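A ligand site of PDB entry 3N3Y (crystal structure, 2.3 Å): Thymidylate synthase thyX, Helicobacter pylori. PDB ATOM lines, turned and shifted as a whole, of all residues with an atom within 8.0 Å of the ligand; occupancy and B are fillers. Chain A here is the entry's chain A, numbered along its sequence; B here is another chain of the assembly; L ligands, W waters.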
ATOM      1  N   ILE A  12     -24.751  18.655 -36.209  1.00  0.00           N
ATOM      2  CA  ILE A  12     -24.070  17.699 -35.331  1.00  0.00           C
ATOM      3  C   ILE A  12     -24.936  17.371 -34.122  1.00  0.00           C
ATOM      4  O   ILE A  12     -25.463  18.274 -33.461  1.00  0.00           O
ATOM      5  CB  ILE A  12     -22.741  18.271 -34.755  1.00  0.00           C
ATOM      6  CG1 ILE A  12     -21.850  18.845 -35.848  1.00  0.00           C
ATOM      7  CG2 ILE A  12     -22.007  17.190 -33.976  1.00  0.00           C
ATOM      8  CD1 ILE A  12     -21.394  17.825 -36.851  1.00  0.00           C
ATOM      9  N   CYS A  13     -25.078  16.087 -33.810  1.00  0.00           N
ATOM     10  CA  CYS A  13     -25.636  15.703 -32.525  1.00  0.00           C
ATOM     11  C   CYS A  13     -24.512  15.570 -31.521  1.00  0.00           C
ATOM     12  O   CYS A  13     -23.696  14.654 -31.623  1.00  0.00           O
ATOM     13  CB  CYS A  13     -26.430  14.410 -32.620  1.00  0.00           C
ATOM     14  SG  CYS A  13     -27.204  13.936 -31.034  1.00  0.00           S
ATOM     15  N   LYS A  14     -24.446  16.486 -30.563  1.00  0.00           N
ATOM     16  CA  LYS A  14     -23.319  16.558 -29.636  1.00  0.00           C
ATOM     17  C   LYS A  14     -23.528  15.706 -28.377  1.00  0.00           C
ATOM     18  O   LYS A  14     -22.581  15.285 -27.727  1.00  0.00           O
ATOM     19  CB  LYS A  14     -23.073  18.019 -29.247  1.00  0.00           C
ATOM     20  CG  LYS A  14     -23.136  18.963 -30.423  1.00  0.00           C
ATOM     21  CD  LYS A  14     -22.515  20.299 -30.074  1.00  0.00           C
ATOM     22  CE  LYS A  14     -23.269  20.960 -28.929  1.00  0.00           C
ATOM     23  NZ  LYS A  14     -22.805  22.383 -28.760  1.00  0.00           N
ATOM     24  N   HIS A  15     -24.784  15.461 -28.016  1.00  0.00           N
ATOM     25  CA  HIS A  15     -25.051  14.594 -26.894  1.00  0.00           C
ATOM     26  C   HIS A  15     -26.450  14.058 -26.980  1.00  0.00           C
ATOM     27  O   HIS A  15     -27.363  14.727 -27.457  1.00  0.00           O
ATOM     28  CB  HIS A  15     -24.854  15.305 -25.554  1.00  0.00           C
ATOM     29  CG  HIS A  15     -24.806  14.358 -24.395  1.00  0.00           C
ATOM     30  ND1 HIS A  15     -23.661  13.695 -24.032  1.00  0.00           N
ATOM     31  CD2 HIS A  15     -25.780  13.929 -23.557  1.00  0.00           C
ATOM     32  CE1 HIS A  15     -23.913  12.914 -23.000  1.00  0.00           C
ATOM     33  NE2 HIS A  15     -25.195  13.036 -22.696  1.00  0.00           N
ATOM     34  N   TYR A  16     -26.627  12.822 -26.533  1.00  0.00           N
ATOM     35  CA  TYR A  16     -27.949  12.210 -26.503  1.00  0.00           C
ATOM     36  C   TYR A  16     -28.115  11.333 -25.277  1.00  0.00           C
ATOM     37  O   TYR A  16     -27.142  10.980 -24.604  1.00  0.00           O
ATOM     38  CB  TYR A  16     -28.225  11.411 -27.776  1.00  0.00           C
ATOM     39  CG  TYR A  16     -27.239  10.291 -28.013  1.00  0.00           C
ATOM     40  CD1 TYR A  16     -27.463   9.013 -27.497  1.00  0.00           C
ATOM     41  CD2 TYR A  16     -26.075  10.514 -28.741  1.00  0.00           C
ATOM     42  CE1 TYR A  16     -26.546   7.985 -27.718  1.00  0.00           C
ATOM     43  CE2 TYR A  16     -25.158   9.493 -28.974  1.00  0.00           C
ATOM     44  CZ  TYR A  16     -25.397   8.238 -28.461  1.00  0.00           C
ATOM     45  OH  TYR A  16     -24.474   7.230 -28.695  1.00  0.00           O
ATOM     46  N   THR A  17     -29.359  10.978 -25.005  1.00  0.00           N
ATOM     47  CA  THR A  17     -29.723  10.203 -23.850  1.00  0.00           C
ATOM     48  C   THR A  17     -29.721   8.728 -24.218  1.00  0.00           C
ATOM     49  O   THR A  17     -30.392   8.323 -25.180  1.00  0.00           O
ATOM     50  CB  THR A  17     -31.134  10.588 -23.330  1.00  0.00           C
ATOM     51  OG1 THR A  17     -31.128  11.947 -22.881  1.00  0.00           O
ATOM     52  CG2 THR A  17     -31.534   9.696 -22.175  1.00  0.00           C
ATOM     53  N   PRO A  18     -28.964   7.911 -23.476  1.00  0.00           N
ATOM     54  CA  PRO A  18     -28.954   6.462 -23.708  1.00  0.00           C
ATOM     55  C   PRO A  18     -30.389   5.963 -23.779  1.00  0.00           C
ATOM     56  O   PRO A  18     -31.203   6.421 -22.986  1.00  0.00           O
ATOM     57  CB  PRO A  18     -28.257   5.909 -22.467  1.00  0.00           C
ATOM     58  CG  PRO A  18     -27.403   7.012 -21.979  1.00  0.00           C
ATOM     59  CD  PRO A  18     -28.105   8.309 -22.349  1.00  0.00           C
ATOM     60  N   LEU A  19     -30.683   5.078 -24.725  1.00  0.00           N
ATOM     61  CA  LEU A  19     -32.024   4.507 -24.867  1.00  0.00           C
ATOM     62  C   LEU A  19     -32.603   3.837 -23.607  1.00  0.00           C
ATOM     63  O   LEU A  19     -33.802   3.828 -23.391  1.00  0.00           O
ATOM     64  CB  LEU A  19     -32.051   3.467 -25.988  1.00  0.00           C
ATOM     65  CG  LEU A  19     -32.377   3.891 -27.420  1.00  0.00           C
ATOM     66  CD1 LEU A  19     -32.404   2.659 -28.309  1.00  0.00           C
ATOM     67  CD2 LEU A  19     -33.703   4.612 -27.495  1.00  0.00           C
ATOM     68  N   ASP A  20     -31.742   3.229 -22.799  1.00  0.00           N
ATOM     69  CA  ASP A  20     -32.221   2.490 -21.634  1.00  0.00           C
ATOM     70  C   ASP A  20     -32.978   3.428 -20.688  1.00  0.00           C
ATOM     71  O   ASP A  20     -33.884   2.989 -19.990  1.00  0.00           O
ATOM     72  CB  ASP A  20     -31.061   1.816 -20.893  1.00  0.00           C
ATOM     73  CG  ASP A  20     -30.018   2.829 -20.417  1.00  0.00           C
ATOM     74  OD1 ASP A  20     -30.071   3.230 -19.235  1.00  0.00           O
ATOM     75  OD2 ASP A  20     -29.155   3.220 -21.255  1.00  0.00           O
ATOM     76  N   ILE A  21     -32.616   4.704 -20.672  1.00  0.00           N
ATOM     77  CA  ILE A  21     -33.370   5.665 -19.885  1.00  0.00           C
ATOM     78  C   ILE A  21     -34.852   5.569 -20.236  1.00  0.00           C
ATOM     79  O   ILE A  21     -35.720   5.559 -19.358  1.00  0.00           O
ATOM     80  CB  ILE A  21     -32.886   7.113 -20.078  1.00  0.00           C
ATOM     81  CG1 ILE A  21     -31.467   7.268 -19.534  1.00  0.00           C
ATOM     82  CG2 ILE A  21     -33.819   8.078 -19.370  1.00  0.00           C
ATOM     83  CD1 ILE A  21     -31.250   6.562 -18.220  1.00  0.00           C
ATOM     84  N   TYR A  64     -33.456  13.040 -24.703  1.00  0.00           N
ATOM     85  CA  TYR A  64     -33.113  14.420 -25.027  1.00  0.00           C
ATOM     86  C   TYR A  64     -31.918  14.493 -25.974  1.00  0.00           C
ATOM     87  O   TYR A  64     -30.944  13.778 -25.813  1.00  0.00           O
ATOM     88  CB  TYR A  64     -32.713  15.131 -23.753  1.00  0.00           C
ATOM     89  CG  TYR A  64     -32.907  16.628 -23.755  1.00  0.00           C
ATOM     90  CD1 TYR A  64     -34.138  17.175 -24.123  1.00  0.00           C
ATOM     91  CD2 TYR A  64     -31.880  17.487 -23.374  1.00  0.00           C
ATOM     92  CE1 TYR A  64     -34.333  18.537 -24.112  1.00  0.00           C
ATOM     93  CE2 TYR A  64     -32.069  18.870 -23.360  1.00  0.00           C
ATOM     94  CZ  TYR A  64     -33.299  19.393 -23.726  1.00  0.00           C
ATOM     95  OH  TYR A  64     -33.514  20.751 -23.708  1.00  0.00           O
ATOM     96  N   TYR A  65     -31.975  15.390 -26.949  1.00  0.00           N
ATOM     97  CA  TYR A  65     -30.882  15.522 -27.923  1.00  0.00           C
ATOM     98  C   TYR A  65     -30.330  16.939 -27.998  1.00  0.00           C
ATOM     99  O   TYR A  65     -31.089  17.884 -28.184  1.00  0.00           O
ATOM    100  CB  TYR A  65     -31.371  15.133 -29.300  1.00  0.00           C
ATOM    101  CG  TYR A  65     -31.940  13.738 -29.325  1.00  0.00           C
ATOM    102  CD1 TYR A  65     -31.101  12.624 -29.462  1.00  0.00           C
ATOM    103  CD2 TYR A  65     -33.302  13.539 -29.211  1.00  0.00           C
ATOM    104  CE1 TYR A  65     -31.627  11.350 -29.493  1.00  0.00           C
ATOM    105  CE2 TYR A  65     -33.834  12.262 -29.236  1.00  0.00           C
ATOM    106  CZ  TYR A  65     -32.989  11.168 -29.368  1.00  0.00           C
ATOM    107  OH  TYR A  65     -33.536   9.915 -29.395  1.00  0.00           O
ATOM    108  N   ASN A  66     -29.017  17.079 -27.834  1.00  0.00           N
ATOM    109  CA  ASN A  66     -28.333  18.343 -28.036  1.00  0.00           C
ATOM    110  C   ASN A  66     -27.657  18.442 -29.401  1.00  0.00           C
ATOM    111  O   ASN A  66     -26.665  17.755 -29.666  1.00  0.00           O
ATOM    112  CB  ASN A  66     -27.281  18.550 -26.947  1.00  0.00           C
ATOM    113  CG  ASN A  66     -27.812  18.251 -25.566  1.00  0.00           C
ATOM    114  OD1 ASN A  66     -27.627  17.155 -25.038  1.00  0.00           O
ATOM    115  ND2 ASN A  66     -28.486  19.232 -24.967  1.00  0.00           N
ATOM    116  N   PRO A 203     -27.798   9.368 -33.486  1.00  0.00           N
ATOM    117  CA  PRO A 203     -27.061   8.094 -33.415  1.00  0.00           C
ATOM    118  C   PRO A 203     -27.887   7.041 -34.146  1.00  0.00           C
ATOM    119  O   PRO A 203     -29.102   7.049 -34.000  1.00  0.00           O
ATOM    120  CB  PRO A 203     -27.044   7.781 -31.913  1.00  0.00           C
ATOM    121  CG  PRO A 203     -27.579   8.996 -31.211  1.00  0.00           C
ATOM    122  CD  PRO A 203     -28.420   9.720 -32.198  1.00  0.00           C
ATOM    123  N   GLU A 205     -28.399   4.054 -33.532  1.00  0.00           N
ATOM    124  CA  GLU A 205     -29.139   3.203 -32.590  1.00  0.00           C
ATOM    125  C   GLU A 205     -30.491   3.794 -32.183  1.00  0.00           C
ATOM    126  O   GLU A 205     -31.402   3.038 -31.815  1.00  0.00           O
ATOM    127  CB  GLU A 205     -28.276   2.857 -31.377  1.00  0.00           C
ATOM    128  CG  GLU A 205     -28.955   3.102 -30.026  1.00  0.00           C
ATOM    129  CD  GLU A 205     -28.947   1.872 -29.119  1.00  0.00           C
ATOM    130  OE1 GLU A 205     -28.674   2.006 -27.894  1.00  0.00           O
ATOM    131  OE2 GLU A 205     -29.220   0.747 -29.631  1.00  0.00           O
ATOM    132  N   HIS A 206     -30.629   5.118 -32.262  1.00  0.00           N
ATOM    133  CA  HIS A 206     -31.910   5.790 -31.968  1.00  0.00           C
ATOM    134  C   HIS A 206     -32.767   6.017 -33.217  1.00  0.00           C
ATOM    135  O   HIS A 206     -33.956   6.327 -33.111  1.00  0.00           O
ATOM    136  CB  HIS A 206     -31.688   7.147 -31.302  1.00  0.00           C
ATOM    137  CG  HIS A 206     -31.175   7.089 -29.890  1.00  0.00           C
ATOM    138  ND1 HIS A 206     -30.083   6.341 -29.525  1.00  0.00           N
ATOM    139  CD2 HIS A 206     -31.569   7.752 -28.785  1.00  0.00           C
ATOM    140  CE1 HIS A 206     -29.840   6.520 -28.240  1.00  0.00           C
ATOM    141  NE2 HIS A 206     -30.723   7.380 -27.767  1.00  0.00           N
ATOM    142  N   HIS B  15     -28.831   9.661 -15.585  1.00  0.00           N
ATOM    143  CA  HIS B  15     -28.048  10.311 -16.637  1.00  0.00           C
ATOM    144  C   HIS B  15     -28.078  11.832 -16.510  1.00  0.00           C
ATOM    145  O   HIS B  15     -29.002  12.403 -15.939  1.00  0.00           O
ATOM    146  CB  HIS B  15     -28.515   9.876 -18.034  1.00  0.00           C
ATOM    147  CG  HIS B  15     -27.586  10.271 -19.134  1.00  0.00           C
ATOM    148  ND1 HIS B  15     -26.584   9.447 -19.601  1.00  0.00           N
ATOM    149  CD2 HIS B  15     -27.487  11.416 -19.867  1.00  0.00           C
ATOM    150  CE1 HIS B  15     -25.911  10.050 -20.560  1.00  0.00           C
ATOM    151  NE2 HIS B  15     -26.442  11.255 -20.738  1.00  0.00           N
ATOM    152  N   TYR B  16     -27.052  12.480 -17.043  1.00  0.00           N
ATOM    153  CA  TYR B  16     -27.010  13.920 -17.032  1.00  0.00           C
ATOM    154  C   TYR B  16     -26.152  14.453 -18.155  1.00  0.00           C
ATOM    155  O   TYR B  16     -25.145  13.852 -18.509  1.00  0.00           O
ATOM    156  CB  TYR B  16     -26.499  14.447 -15.691  1.00  0.00           C
ATOM    157  CG  TYR B  16     -25.066  14.075 -15.394  1.00  0.00           C
ATOM    158  CD1 TYR B  16     -24.009  14.859 -15.859  1.00  0.00           C
ATOM    159  CD2 TYR B  16     -24.768  12.934 -14.662  1.00  0.00           C
ATOM    160  CE1 TYR B  16     -22.706  14.520 -15.587  1.00  0.00           C
ATOM    161  CE2 TYR B  16     -23.457  12.583 -14.388  1.00  0.00           C
ATOM    162  CZ  TYR B  16     -22.429  13.374 -14.848  1.00  0.00           C
ATOM    163  OH  TYR B  16     -21.124  13.019 -14.569  1.00  0.00           O
ATOM    164  N   PRO B  18     -23.452  16.651 -20.057  1.00  0.00           N
ATOM    165  CA  PRO B  18     -22.149  17.222 -19.701  1.00  0.00           C
ATOM    166  C   PRO B  18     -22.203  18.745 -19.678  1.00  0.00           C
ATOM    167  O   PRO B  18     -22.837  19.335 -20.540  1.00  0.00           O
ATOM    168  CB  PRO B  18     -21.227  16.740 -20.824  1.00  0.00           C
ATOM    169  CG  PRO B  18     -21.904  15.583 -21.427  1.00  0.00           C
ATOM    170  CD  PRO B  18     -23.378  15.805 -21.268  1.00  0.00           C
ATOM    171  N   ILE B  21     -21.835  21.151 -22.932  1.00  0.00           N
ATOM    172  CA  ILE B  21     -22.996  21.393 -23.766  1.00  0.00           C
ATOM    173  C   ILE B  21     -23.570  22.791 -23.503  1.00  0.00           C
ATOM    174  O   ILE B  21     -23.867  23.535 -24.449  1.00  0.00           O
ATOM    175  CB  ILE B  21     -24.087  20.328 -23.576  1.00  0.00           C
ATOM    176  CG1 ILE B  21     -23.612  18.971 -24.096  1.00  0.00           C
ATOM    177  CG2 ILE B  21     -25.383  20.762 -24.292  1.00  0.00           C
ATOM    178  CD1 ILE B  21     -23.281  18.970 -25.591  1.00  0.00           C
HETATM  179  N1  LIG L   1     -22.583   9.838 -26.424  1.00  0.00           N
HETATM  180  C1  LIG L   1     -23.705  10.413 -25.875  1.00  0.00           C
HETATM  181  N2  LIG L   1     -24.544   9.663 -25.074  1.00  0.00           N
HETATM  182  C2  LIG L   1     -24.254   8.340 -24.846  1.00  0.00           C
HETATM  183  C3  LIG L   1     -23.118   7.757 -25.401  1.00  0.00           C
HETATM  184  C4  LIG L   1     -22.286   8.518 -26.203  1.00  0.00           C
HETATM  185  O1  LIG L   1     -23.959  11.600 -26.084  1.00  0.00           O
HETATM  186  O2  LIG L   1     -25.009   7.696 -24.143  1.00  0.00           O
HETATM  187  C5  LIG L   1     -21.721  10.683 -27.269  1.00  0.00           C
HETATM  188  C6  LIG L   1     -20.391  10.967 -26.614  1.00  0.00           C
HETATM  189  C7  LIG L   1     -19.505  11.181 -27.825  1.00  0.00           C
HETATM  190  C8  LIG L   1     -20.187  10.474 -28.984  1.00  0.00           C
HETATM  191  O3  LIG L   1     -19.408  12.559 -28.081  1.00  0.00           O
HETATM  192  O4  LIG L   1     -21.477  10.103 -28.547  1.00  0.00           O
HETATM  193  C9  LIG L   1     -19.417   9.224 -29.391  1.00  0.00           C
HETATM  194  O5  LIG L   1     -19.324   8.354 -28.280  1.00  0.00           O
HETATM  195  P1  LIG L   1     -18.840   6.821 -28.436  1.00  0.00           P
HETATM  196  O6  LIG L   1     -19.196   6.085 -27.168  1.00  0.00           O
HETATM  197  O7  LIG L   1     -17.336   6.837 -28.606  1.00  0.00           O
HETATM  198  O8  LIG L   1     -19.513   6.204 -29.593  1.00  0.00           O
HETATM  199  O   HOH W   1     -23.347  12.257 -30.016  1.00  0.00           O
HETATM  200  O   HOH W   2     -22.351   7.615 -30.300  1.00  0.00           O
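A ring nitrogen (ND1) of His 15 of chain A is in hydrogen-bond range of an oxygen (O1) of the ligand, at 2.9 Å. N of Tyr 16 of chain A sits at hydrogen-bond distance from O1 of the ligand, 3.0 Å away. The backbone carbonyl oxygen of Tyr 16 of chain A lies within hydrogen-bond range of a nitrogen (N2) of the ligand (3.0 Å).
A ring nitrogen (NE2) of His 15 of chain B sits at hydrogen-bond distance from a ring nitrogen (NE2) of His 15 of chain A. The backbone carbonyl oxygen of His 15 of chain A is in hydrogen-bond range of the side-chain sulfur of Cys 13 (3.7 Å). The backbone NH (N) of Asn 66 is in hydrogen-bond range of the backbone carbonyl oxygen (O) of His 15 of chain A (2.9 Å).
Residues that only touch the ligand: Pro 18 of chain A. Hydrophobic or aromatic side chains that line the ligand: His 15 of chain A, Tyr 16 of chain A and Pro 18 of chain A. Of the 20 residues printed, 3 come within 4 Å of the ligand. The nearest printed residue that does not touch the ligand is Lys 14 (4.2 Å).
Water W2 lies within hydrogen-bond range of OH of Tyr 16 of chain A (2.7 Å) and O4 of the ligand (3.2 Å). Water W1 lies within hydrogen-bond range of O of Cys 13 (2.9 Å) and O4 of the ligand (3.2 Å).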
